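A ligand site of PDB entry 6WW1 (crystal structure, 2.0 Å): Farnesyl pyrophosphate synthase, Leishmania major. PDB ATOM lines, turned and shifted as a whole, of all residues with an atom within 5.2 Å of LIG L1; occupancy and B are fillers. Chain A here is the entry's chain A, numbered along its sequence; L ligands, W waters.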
ATOM      1  N   GLY A  46      -8.088  33.561  14.509  1.00  0.00           N
ATOM      2  CA  GLY A  46      -8.797  32.947  13.396  1.00  0.00           C
ATOM      3  C   GLY A  46      -9.168  31.512  13.689  1.00  0.00           C
ATOM      4  O   GLY A  46      -9.768  30.842  12.871  1.00  0.00           O
ATOM      5  N   GLY A  47      -8.813  31.021  14.869  1.00  0.00           N
ATOM      6  CA  GLY A  47      -9.214  29.659  15.258  1.00  0.00           C
ATOM      7  C   GLY A  47     -10.548  29.700  15.964  1.00  0.00           C
ATOM      8  O   GLY A  47     -11.200  30.737  16.031  1.00  0.00           O
ATOM      9  N   LYS A  48     -10.981  28.565  16.505  1.00  0.00           N
ATOM     10  CA  LYS A  48     -12.319  28.581  17.143  1.00  0.00           C
ATOM     11  C   LYS A  48     -12.213  29.078  18.582  1.00  0.00           C
ATOM     12  O   LYS A  48     -13.206  29.323  19.232  1.00  0.00           O
ATOM     13  CB  LYS A  48     -12.906  27.185  17.166  1.00  0.00           C
ATOM     14  CG  LYS A  48     -13.054  26.509  15.801  1.00  0.00           C
ATOM     15  CD  LYS A  48     -13.438  25.016  15.946  1.00  0.00           C
ATOM     16  CE  LYS A  48     -12.229  24.072  16.085  1.00  0.00           C
ATOM     17  NZ  LYS A  48     -11.356  24.052  14.832  1.00  0.00           N
ATOM     18  N   TYR A  49     -10.989  29.137  19.104  1.00  0.00           N
ATOM     19  CA  TYR A  49     -10.669  29.485  20.512  1.00  0.00           C
ATOM     20  C   TYR A  49     -11.302  28.498  21.518  1.00  0.00           C
ATOM     21  O   TYR A  49     -11.569  28.909  22.649  1.00  0.00           O
ATOM     22  CB  TYR A  49     -11.067  30.901  20.931  1.00  0.00           C
ATOM     23  CG  TYR A  49     -10.624  32.108  20.154  1.00  0.00           C
ATOM     24  CD1 TYR A  49      -9.483  32.135  19.382  1.00  0.00           C
ATOM     25  CD2 TYR A  49     -11.291  33.293  20.338  1.00  0.00           C
ATOM     26  CE1 TYR A  49      -9.064  33.289  18.763  1.00  0.00           C
ATOM     27  CE2 TYR A  49     -10.901  34.449  19.724  1.00  0.00           C
ATOM     28  CZ  TYR A  49      -9.803  34.435  18.900  1.00  0.00           C
ATOM     29  OH  TYR A  49      -9.431  35.595  18.344  1.00  0.00           O
ATOM     30  N   ARG A  51      -9.918  26.080  23.326  1.00  0.00           N
ATOM     31  CA  ARG A  51      -8.980  25.944  24.468  1.00  0.00           C
ATOM     32  C   ARG A  51      -9.049  27.189  25.373  1.00  0.00           C
ATOM     33  O   ARG A  51      -9.293  27.037  26.486  1.00  0.00           O
ATOM     34  CB  ARG A  51      -7.569  25.707  23.930  1.00  0.00           C
ATOM     35  CG  ARG A  51      -7.401  24.470  23.071  1.00  0.00           C
ATOM     36  CD  ARG A  51      -6.028  24.458  22.438  1.00  0.00           C
ATOM     37  NE  ARG A  51      -5.905  23.347  21.541  1.00  0.00           N
ATOM     38  CZ  ARG A  51      -6.509  23.233  20.364  1.00  0.00           C
ATOM     39  NH1 ARG A  51      -7.248  24.204  19.861  1.00  0.00           N
ATOM     40  NH2 ARG A  51      -6.333  22.146  19.657  1.00  0.00           N
ATOM     41  N   GLU A  88      -3.802  29.337  23.584  1.00  0.00           N
ATOM     42  CA  GLU A  88      -3.938  29.801  22.179  1.00  0.00           C
ATOM     43  C   GLU A  88      -2.547  30.141  21.646  1.00  0.00           C
ATOM     44  O   GLU A  88      -2.287  29.811  20.532  1.00  0.00           O
ATOM     45  CB  GLU A  88      -4.862  31.011  22.077  1.00  0.00           C
ATOM     46  CG  GLU A  88      -6.309  30.724  22.458  1.00  0.00           C
ATOM     47  CD  GLU A  88      -6.928  29.629  21.613  1.00  0.00           C
ATOM     48  OE1 GLU A  88      -6.657  29.604  20.390  1.00  0.00           O
ATOM     49  OE2 GLU A  88      -7.674  28.796  22.164  1.00  0.00           O
ATOM     50  N   GLN A  91      -0.796  26.759  21.084  1.00  0.00           N
ATOM     51  CA  GLN A  91      -1.435  26.237  19.844  1.00  0.00           C
ATOM     52  C   GLN A  91      -0.792  26.951  18.647  1.00  0.00           C
ATOM     53  O   GLN A  91      -0.327  26.280  17.789  1.00  0.00           O
ATOM     54  CB  GLN A  91      -2.942  26.491  19.890  1.00  0.00           C
ATOM     55  CG  GLN A  91      -3.599  26.411  18.534  1.00  0.00           C
ATOM     56  CD  GLN A  91      -3.935  24.986  18.152  1.00  0.00           C
ATOM     57  OE1 GLN A  91      -5.010  24.702  17.631  1.00  0.00           O
ATOM     58  NE2 GLN A  91      -2.979  24.110  18.390  1.00  0.00           N
ATOM     59  N   LEU A  95       1.144  24.977  15.719  1.00  0.00           N
ATOM     60  CA  LEU A  95       0.713  24.947  14.322  1.00  0.00           C
ATOM     61  C   LEU A  95       1.717  25.594  13.374  1.00  0.00           C
ATOM     62  O   LEU A  95       1.799  25.181  12.191  1.00  0.00           O
ATOM     63  CB  LEU A  95      -0.681  25.545  14.136  1.00  0.00           C
ATOM     64  CG  LEU A  95      -1.797  25.052  15.060  1.00  0.00           C
ATOM     65  CD1 LEU A  95      -3.148  25.712  14.727  1.00  0.00           C
ATOM     66  CD2 LEU A  95      -1.856  23.518  15.032  1.00  0.00           C
ATOM     67  N   ARG A 107      -3.720  27.450   6.654  1.00  0.00           N
ATOM     68  CA  ARG A 107      -4.152  27.275   8.047  1.00  0.00           C
ATOM     69  C   ARG A 107      -5.215  28.344   8.284  1.00  0.00           C
ATOM     70  O   ARG A 107      -4.989  29.525   7.945  1.00  0.00           O
ATOM     71  CB  ARG A 107      -2.985  27.516   9.044  1.00  0.00           C
ATOM     72  CG  ARG A 107      -3.479  27.617  10.483  1.00  0.00           C
ATOM     73  CD  ARG A 107      -3.960  26.266  11.000  1.00  0.00           C
ATOM     74  NE  ARG A 107      -2.910  25.234  10.960  1.00  0.00           N
ATOM     75  CZ  ARG A 107      -3.123  23.951  11.287  1.00  0.00           C
ATOM     76  NH1 ARG A 107      -4.364  23.552  11.732  1.00  0.00           N
ATOM     77  NH2 ARG A 107      -2.102  23.086  11.246  1.00  0.00           N
ATOM     78  N   ARG A 108      -6.363  27.929   8.850  1.00  0.00           N
ATOM     79  CA  ARG A 108      -7.485  28.837   9.175  1.00  0.00           C
ATOM     80  C   ARG A 108      -7.887  29.739   7.991  1.00  0.00           C
ATOM     81  O   ARG A 108      -8.083  30.940   8.162  1.00  0.00           O
ATOM     82  CB  ARG A 108      -7.164  29.700  10.386  1.00  0.00           C
ATOM     83  CG  ARG A 108      -7.070  28.897  11.664  1.00  0.00           C
ATOM     84  CD  ARG A 108      -6.176  29.606  12.691  1.00  0.00           C
ATOM     85  NE  ARG A 108      -6.112  28.913  13.966  1.00  0.00           N
ATOM     86  CZ  ARG A 108      -5.333  29.256  14.982  1.00  0.00           C
ATOM     87  NH1 ARG A 108      -4.525  30.291  14.851  1.00  0.00           N
ATOM     88  NH2 ARG A 108      -5.359  28.562  16.119  1.00  0.00           N
ATOM     89  N   THR A 208      -2.430  15.615  21.340  1.00  0.00           N
ATOM     90  CA  THR A 208      -3.661  16.358  21.241  1.00  0.00           C
ATOM     91  C   THR A 208      -4.391  16.501  22.561  1.00  0.00           C
ATOM     92  O   THR A 208      -4.647  17.612  22.921  1.00  0.00           O
ATOM     93  CB  THR A 208      -4.612  15.850  20.140  1.00  0.00           C
ATOM     94  OG1 THR A 208      -4.025  16.192  18.881  1.00  0.00           O
ATOM     95  CG2 THR A 208      -5.966  16.620  20.210  1.00  0.00           C
ATOM     96  N   TYR A 211      -2.967  18.904  25.697  1.00  0.00           N
ATOM     97  CA  TYR A 211      -2.986  20.366  25.547  1.00  0.00           C
ATOM     98  C   TYR A 211      -4.347  20.950  25.133  1.00  0.00           C
ATOM     99  O   TYR A 211      -4.594  22.176  25.353  1.00  0.00           O
ATOM    100  CB  TYR A 211      -1.885  20.847  24.582  1.00  0.00           C
ATOM    101  CG  TYR A 211      -2.249  21.013  23.093  1.00  0.00           C
ATOM    102  CD1 TYR A 211      -2.146  19.954  22.204  1.00  0.00           C
ATOM    103  CD2 TYR A 211      -2.551  22.309  22.562  1.00  0.00           C
ATOM    104  CE1 TYR A 211      -2.416  20.118  20.835  1.00  0.00           C
ATOM    105  CE2 TYR A 211      -2.814  22.478  21.193  1.00  0.00           C
ATOM    106  CZ  TYR A 211      -2.728  21.362  20.341  1.00  0.00           C
ATOM    107  OH  TYR A 211      -2.955  21.521  19.011  1.00  0.00           O
ATOM    108  N   THR A 212      -5.183  20.119  24.516  1.00  0.00           N
ATOM    109  CA  THR A 212      -6.481  20.591  24.007  1.00  0.00           C
ATOM    110  C   THR A 212      -7.630  20.386  25.023  1.00  0.00           C
ATOM    111  O   THR A 212      -8.586  21.164  25.038  1.00  0.00           O
ATOM    112  CB  THR A 212      -6.873  19.962  22.653  1.00  0.00           C
ATOM    113  OG1 THR A 212      -5.807  20.136  21.731  1.00  0.00           O
ATOM    114  CG2 THR A 212      -8.144  20.629  22.077  1.00  0.00           C
ATOM    115  N   PHE A 246     -11.671  13.969  19.884  1.00  0.00           N
ATOM    116  CA  PHE A 246     -11.459  15.206  19.154  1.00  0.00           C
ATOM    117  C   PHE A 246     -10.454  14.993  18.007  1.00  0.00           C
ATOM    118  O   PHE A 246     -10.624  15.529  16.924  1.00  0.00           O
ATOM    119  CB  PHE A 246     -10.992  16.304  20.085  1.00  0.00           C
ATOM    120  CG  PHE A 246     -10.646  17.601  19.389  1.00  0.00           C
ATOM    121  CD1 PHE A 246      -9.349  17.836  18.878  1.00  0.00           C
ATOM    122  CD2 PHE A 246     -11.610  18.618  19.271  1.00  0.00           C
ATOM    123  CE1 PHE A 246      -9.034  19.030  18.244  1.00  0.00           C
ATOM    124  CE2 PHE A 246     -11.311  19.830  18.653  1.00  0.00           C
ATOM    125  CZ  PHE A 246     -10.016  20.037  18.104  1.00  0.00           C
ATOM    126  N   GLN A 247      -9.421  14.179  18.268  1.00  0.00           N
ATOM    127  CA  GLN A 247      -8.381  13.862  17.258  1.00  0.00           C
ATOM    128  C   GLN A 247      -8.995  12.947  16.189  1.00  0.00           C
ATOM    129  O   GLN A 247      -8.657  13.117  14.997  1.00  0.00           O
ATOM    130  CB  GLN A 247      -7.178  13.191  17.926  1.00  0.00           C
ATOM    131  CG  GLN A 247      -5.889  13.309  17.114  1.00  0.00           C
ATOM    132  CD  GLN A 247      -5.826  14.608  16.348  1.00  0.00           C
ATOM    133  OE1 GLN A 247      -5.783  15.695  16.918  1.00  0.00           O
ATOM    134  NE2 GLN A 247      -5.814  14.502  15.030  1.00  0.00           N
ATOM    135  N   ASP A 250     -10.837  14.994  13.807  1.00  0.00           N
ATOM    136  CA  ASP A 250      -9.846  15.742  12.995  1.00  0.00           C
ATOM    137  C   ASP A 250      -9.280  14.803  11.920  1.00  0.00           C
ATOM    138  O   ASP A 250      -8.926  15.295  10.832  1.00  0.00           O
ATOM    139  CB  ASP A 250      -8.742  16.343  13.870  1.00  0.00           C
ATOM    140  CG  ASP A 250      -7.825  17.291  13.115  1.00  0.00           C
ATOM    141  OD1 ASP A 250      -8.352  18.255  12.516  1.00  0.00           O
ATOM    142  OD2 ASP A 250      -6.596  17.075  13.149  1.00  0.00           O
ATOM    143  N   LYS A 264      -8.257  24.300   6.120  1.00  0.00           N
ATOM    144  CA  LYS A 264      -6.938  23.705   5.963  1.00  0.00           C
ATOM    145  C   LYS A 264      -7.027  22.534   4.956  1.00  0.00           C
ATOM    146  O   LYS A 264      -8.110  22.010   4.740  1.00  0.00           O
ATOM    147  CB  LYS A 264      -6.419  23.236   7.323  1.00  0.00           C
ATOM    148  CG  LYS A 264      -7.290  22.179   7.991  1.00  0.00           C
ATOM    149  CD  LYS A 264      -6.815  21.951   9.406  1.00  0.00           C
ATOM    150  CE  LYS A 264      -7.507  20.700   9.962  1.00  0.00           C
ATOM    151  NZ  LYS A 264      -7.364  20.570  11.448  1.00  0.00           N
ATOM    152  N   ARG A 360     -19.078  18.403  16.133  1.00  0.00           N
ATOM    153  CA  ARG A 360     -18.556  19.593  15.475  1.00  0.00           C
ATOM    154  C   ARG A 360     -18.306  19.241  14.013  1.00  0.00           C
ATOM    155  O   ARG A 360     -18.166  18.064  13.644  1.00  0.00           O
ATOM    156  CB  ARG A 360     -17.226  20.069  16.102  1.00  0.00           C
ATOM    157  CG  ARG A 360     -16.093  19.068  15.928  1.00  0.00           C
ATOM    158  CD  ARG A 360     -14.910  19.446  16.834  1.00  0.00           C
ATOM    159  NE  ARG A 360     -13.704  18.636  16.580  1.00  0.00           N
ATOM    160  CZ  ARG A 360     -12.686  19.009  15.812  1.00  0.00           C
ATOM    161  NH1 ARG A 360     -12.677  20.170  15.152  1.00  0.00           N
ATOM    162  NH2 ARG A 360     -11.648  18.187  15.685  1.00  0.00           N
ATOM    163  N   LYS A 362     -16.105  21.459  12.103  1.00  0.00           N
ATOM    164  CA  LYS A 362     -14.760  21.963  11.782  1.00  0.00           C
ATOM    165  C   LYS A 362     -13.974  22.171  13.047  1.00  0.00           C
ATOM    166  O   LYS A 362     -12.828  22.561  12.926  1.00  0.00           O
ATOM    167  CB  LYS A 362     -14.808  23.296  11.001  1.00  0.00           C
ATOM    168  CG  LYS A 362     -15.731  24.365  11.581  1.00  0.00           C
ATOM    169  CD  LYS A 362     -15.405  25.742  10.972  1.00  0.00           C
ATOM    170  CE  LYS A 362     -14.179  26.331  11.686  1.00  0.00           C
ATOM    171  NZ  LYS A 362     -13.682  27.606  11.102  1.00  0.00           N
ATOM    172  OXT LYS A 362     -14.492  21.995  14.158  1.00  0.00           O
HETATM  173  P1  LIG L   1      -8.155  26.117  15.783  1.00  0.00           P
HETATM  174  O1  LIG L   1      -7.767  26.745  14.422  1.00  0.00           O
HETATM  175  O2  LIG L   1      -9.622  26.210  16.201  1.00  0.00           O
HETATM  176  O3  LIG L   1      -7.212  26.530  16.908  1.00  0.00           O
HETATM  177  O4  LIG L   1      -7.634  24.584  15.650  1.00  0.00           O
HETATM  178  P2  LIG L   1      -8.204  23.194  16.292  1.00  0.00           P
HETATM  179  O5  LIG L   1      -9.087  22.488  15.245  1.00  0.00           O
HETATM  180  O6  LIG L   1      -8.758  23.379  17.646  1.00  0.00           O
HETATM  181  O7  LIG L   1      -6.876  22.339  16.508  1.00  0.00           O
HETATM  182  C1  LIG L   1      -6.110  21.970  15.366  1.00  0.00           C
HETATM  183  C2  LIG L   1      -5.116  21.040  16.019  1.00  0.00           C
HETATM  184  C3  LIG L   1      -5.456  19.557  16.202  1.00  0.00           C
HETATM  185  C4  LIG L   1      -5.439  19.164  17.646  1.00  0.00           C
HETATM  186  C5  LIG L   1      -6.741  19.002  15.544  1.00  0.00           C
HETATM  187  O1  LG2 L   2      -4.496  20.852  12.354  1.00  0.00           O
HETATM  188  P1  LG2 L   2      -3.771  19.725  11.626  1.00  0.00           P
HETATM  189  O2  LG2 L   2      -2.562  20.243  10.909  1.00  0.00           O
HETATM  190  O3  LG2 L   2      -4.691  18.781  10.889  1.00  0.00           O
HETATM  191  C1  LG2 L   2      -3.107  18.676  12.961  1.00  0.00           C
HETATM  192  P2  LG2 L   2      -2.298  17.117  12.503  1.00  0.00           P
HETATM  193  O4  LG2 L   2      -1.079  17.402  11.672  1.00  0.00           O
HETATM  194  O5  LG2 L   2      -1.920  16.491  13.843  1.00  0.00           O
HETATM  195  O6  LG2 L   2      -3.416  16.268  11.922  1.00  0.00           O
HETATM  196  C2  LG2 L   2      -2.072  19.491  13.708  1.00  0.00           C
HETATM  197  N1  LG2 L   2      -1.666  19.117  15.073  1.00  0.00           N
HETATM  198  C3  LG2 L   2      -0.415  19.540  15.408  1.00  0.00           C
HETATM  199  C4  LG2 L   2       0.193  19.304  16.642  1.00  0.00           C
HETATM  200  C5  LG2 L   2      -0.576  18.620  17.596  1.00  0.00           C
HETATM  201  C6  LG2 L   2      -1.892  18.178  17.294  1.00  0.00           C
HETATM  202  C7  LG2 L   2      -2.422  18.449  15.996  1.00  0.00           C
HETATM  203  C8  LG2 L   2       1.632  19.822  16.839  1.00  0.00           C
HETATM  204  C9  LG2 L   2       2.440  19.159  17.941  1.00  0.00           C
HETATM  205  C10 LG2 L   2       3.749  19.878  18.227  1.00  0.00           C
HETATM  206  C11 LG2 L   2       4.513  20.324  16.972  1.00  0.00           C
HETATM  207  O   HOH W   1      -8.437  22.636  12.723  1.00  0.00           O
HETATM  208  O   HOH W   2      -9.921  19.765  14.300  1.00  0.00           O
HETATM  209  O   HOH W   3     -10.378  26.501  13.133  1.00  0.00           O
HETATM  210  O   HOH W   4     -10.195  25.890  19.093  1.00  0.00           O
HETATM  211  O   HOH W   5      -6.781  24.973  12.539  1.00  0.00           O
HETATM  212  O   HOH W   6      -8.283  28.569  18.486  1.00  0.00           O
HETATM  213  O   HOH W   7     -10.535  23.118  19.373  1.00  0.00           O
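NZ of Lys 264 is in salt-bridge range of O1 of LG2 L2 (3.0 Å).
NE of Arg 108 is in salt-bridge range of O1 of LIG L1 (2.8 Å).
The guanidinium group of Arg 51 is in salt-bridge range of an oxygen (O6) of LIG L1 (2.8 Å).
The guanidinium group (NH1) of Arg 107 is in salt-bridge range of an oxygen (O1) of LG2 L2 (2.8 Å).
The backbone NH (N) of Lys 48 lies within hydrogen-bond range of an oxygen (O2) of LIG L1, 2.7 Å away.
The side-chain amide oxygen (OE1) of Gln 91 lies close to an oxygen (O3) of LIG L1.
An oxygen (O5) of LIG L1 is in salt-bridge range of the side-chain amino group (NZ) of Lys 48, 2.8 Å away.
The backbone carbonyl oxygen (O) of Thr 208 lies within hydrogen-bond range of the side-chain hydroxyl (OG1) of Thr 212 (3.0 Å).
The guanidinium group (NH2) of Arg 51 sits at hydrogen-bond distance from the side-chain hydroxyl (OG1) of Thr 212.
OD1 of Asp 250 lies within salt-bridge range of NZ of Lys 264 (2.7 Å).
The side-chain carboxylate (OD2) of Asp 250 lies close to the side-chain amide nitrogen (NE2) of Gln 247 (3.3 Å).
The side-chain amide nitrogen (NE2) of Gln 91 sits at hydrogen-bond distance from the side-chain hydroxyl (OH) of Tyr 211, at 2.7 Å.
OE1 of Gln 247 is in hydrogen-bond range of OG1 of Thr 208.
The side-chain amino group (NZ) of Lys 48 is in salt-bridge range of the chain-end carboxylate (O) of Lys 362 (2.8 Å).
The side-chain amide oxygen of Gln 91 sits at hydrogen-bond distance from the guanidinium group of Arg 51 (3.2 Å).
CA of Gly 47 touches O1 of LIG L1 (3.4 Å).
Thr 208 touches LIG L1.
OH of Tyr 211 touches C4 of LIG L1, 3.7 Å away.
CE1 of Phe 246 touches C5 of LIG L1 (3.5 Å).
Gln 247 touches LIG L1.
Asp 250 touches LIG L1.
Hydrophobic or aromatic side chains that line LIG L1: Phe 246.
Within 4 Å of LIG L1: Gly 47, Lys 48, Arg 51, Gln 91, Arg 108, Thr 208, Tyr 211, Phe 246, Gln 247 and Asp 250.
Along chain A the residues within 4 Å of LIG L1 span positions 47 to 250.
Water W7 bridges O6 of LIG L1 (2.5 Å) and NH1 of Arg 51 (3.5 Å).
Water W1 lies within hydrogen-bond range of O5 of LIG L1 (2.6 Å) and NZ of Lys 264 (2.7 Å).
Water W6 lies within hydrogen-bond range of the side-chain carboxylate of Glu 88 (2.7 Å), an oxygen (O3) of LIG L1 (2.8 Å), the backbone NH of Tyr 49 (2.8 Å) and the backbone NH of Lys 48 (3.3 Å).
Water W3 lies within hydrogen-bond range of an oxygen (O1) of LIG L1 and the side-chain amino group (NZ) of Lys 48.
Water W4 lies within hydrogen-bond range of an oxygen (O2) of LIG L1 (3.0 Å), the backbone NH (N) of Tyr 49 (3.3 Å) and the guanidinium group (NH1) of Arg 51 (3.5 Å).
Water W2 lies within hydrogen-bond range of the guanidinium group (NH2) of Arg 360, the side-chain carboxylate (OD1) of Asp 250 and an oxygen (O5) of LIG L1.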
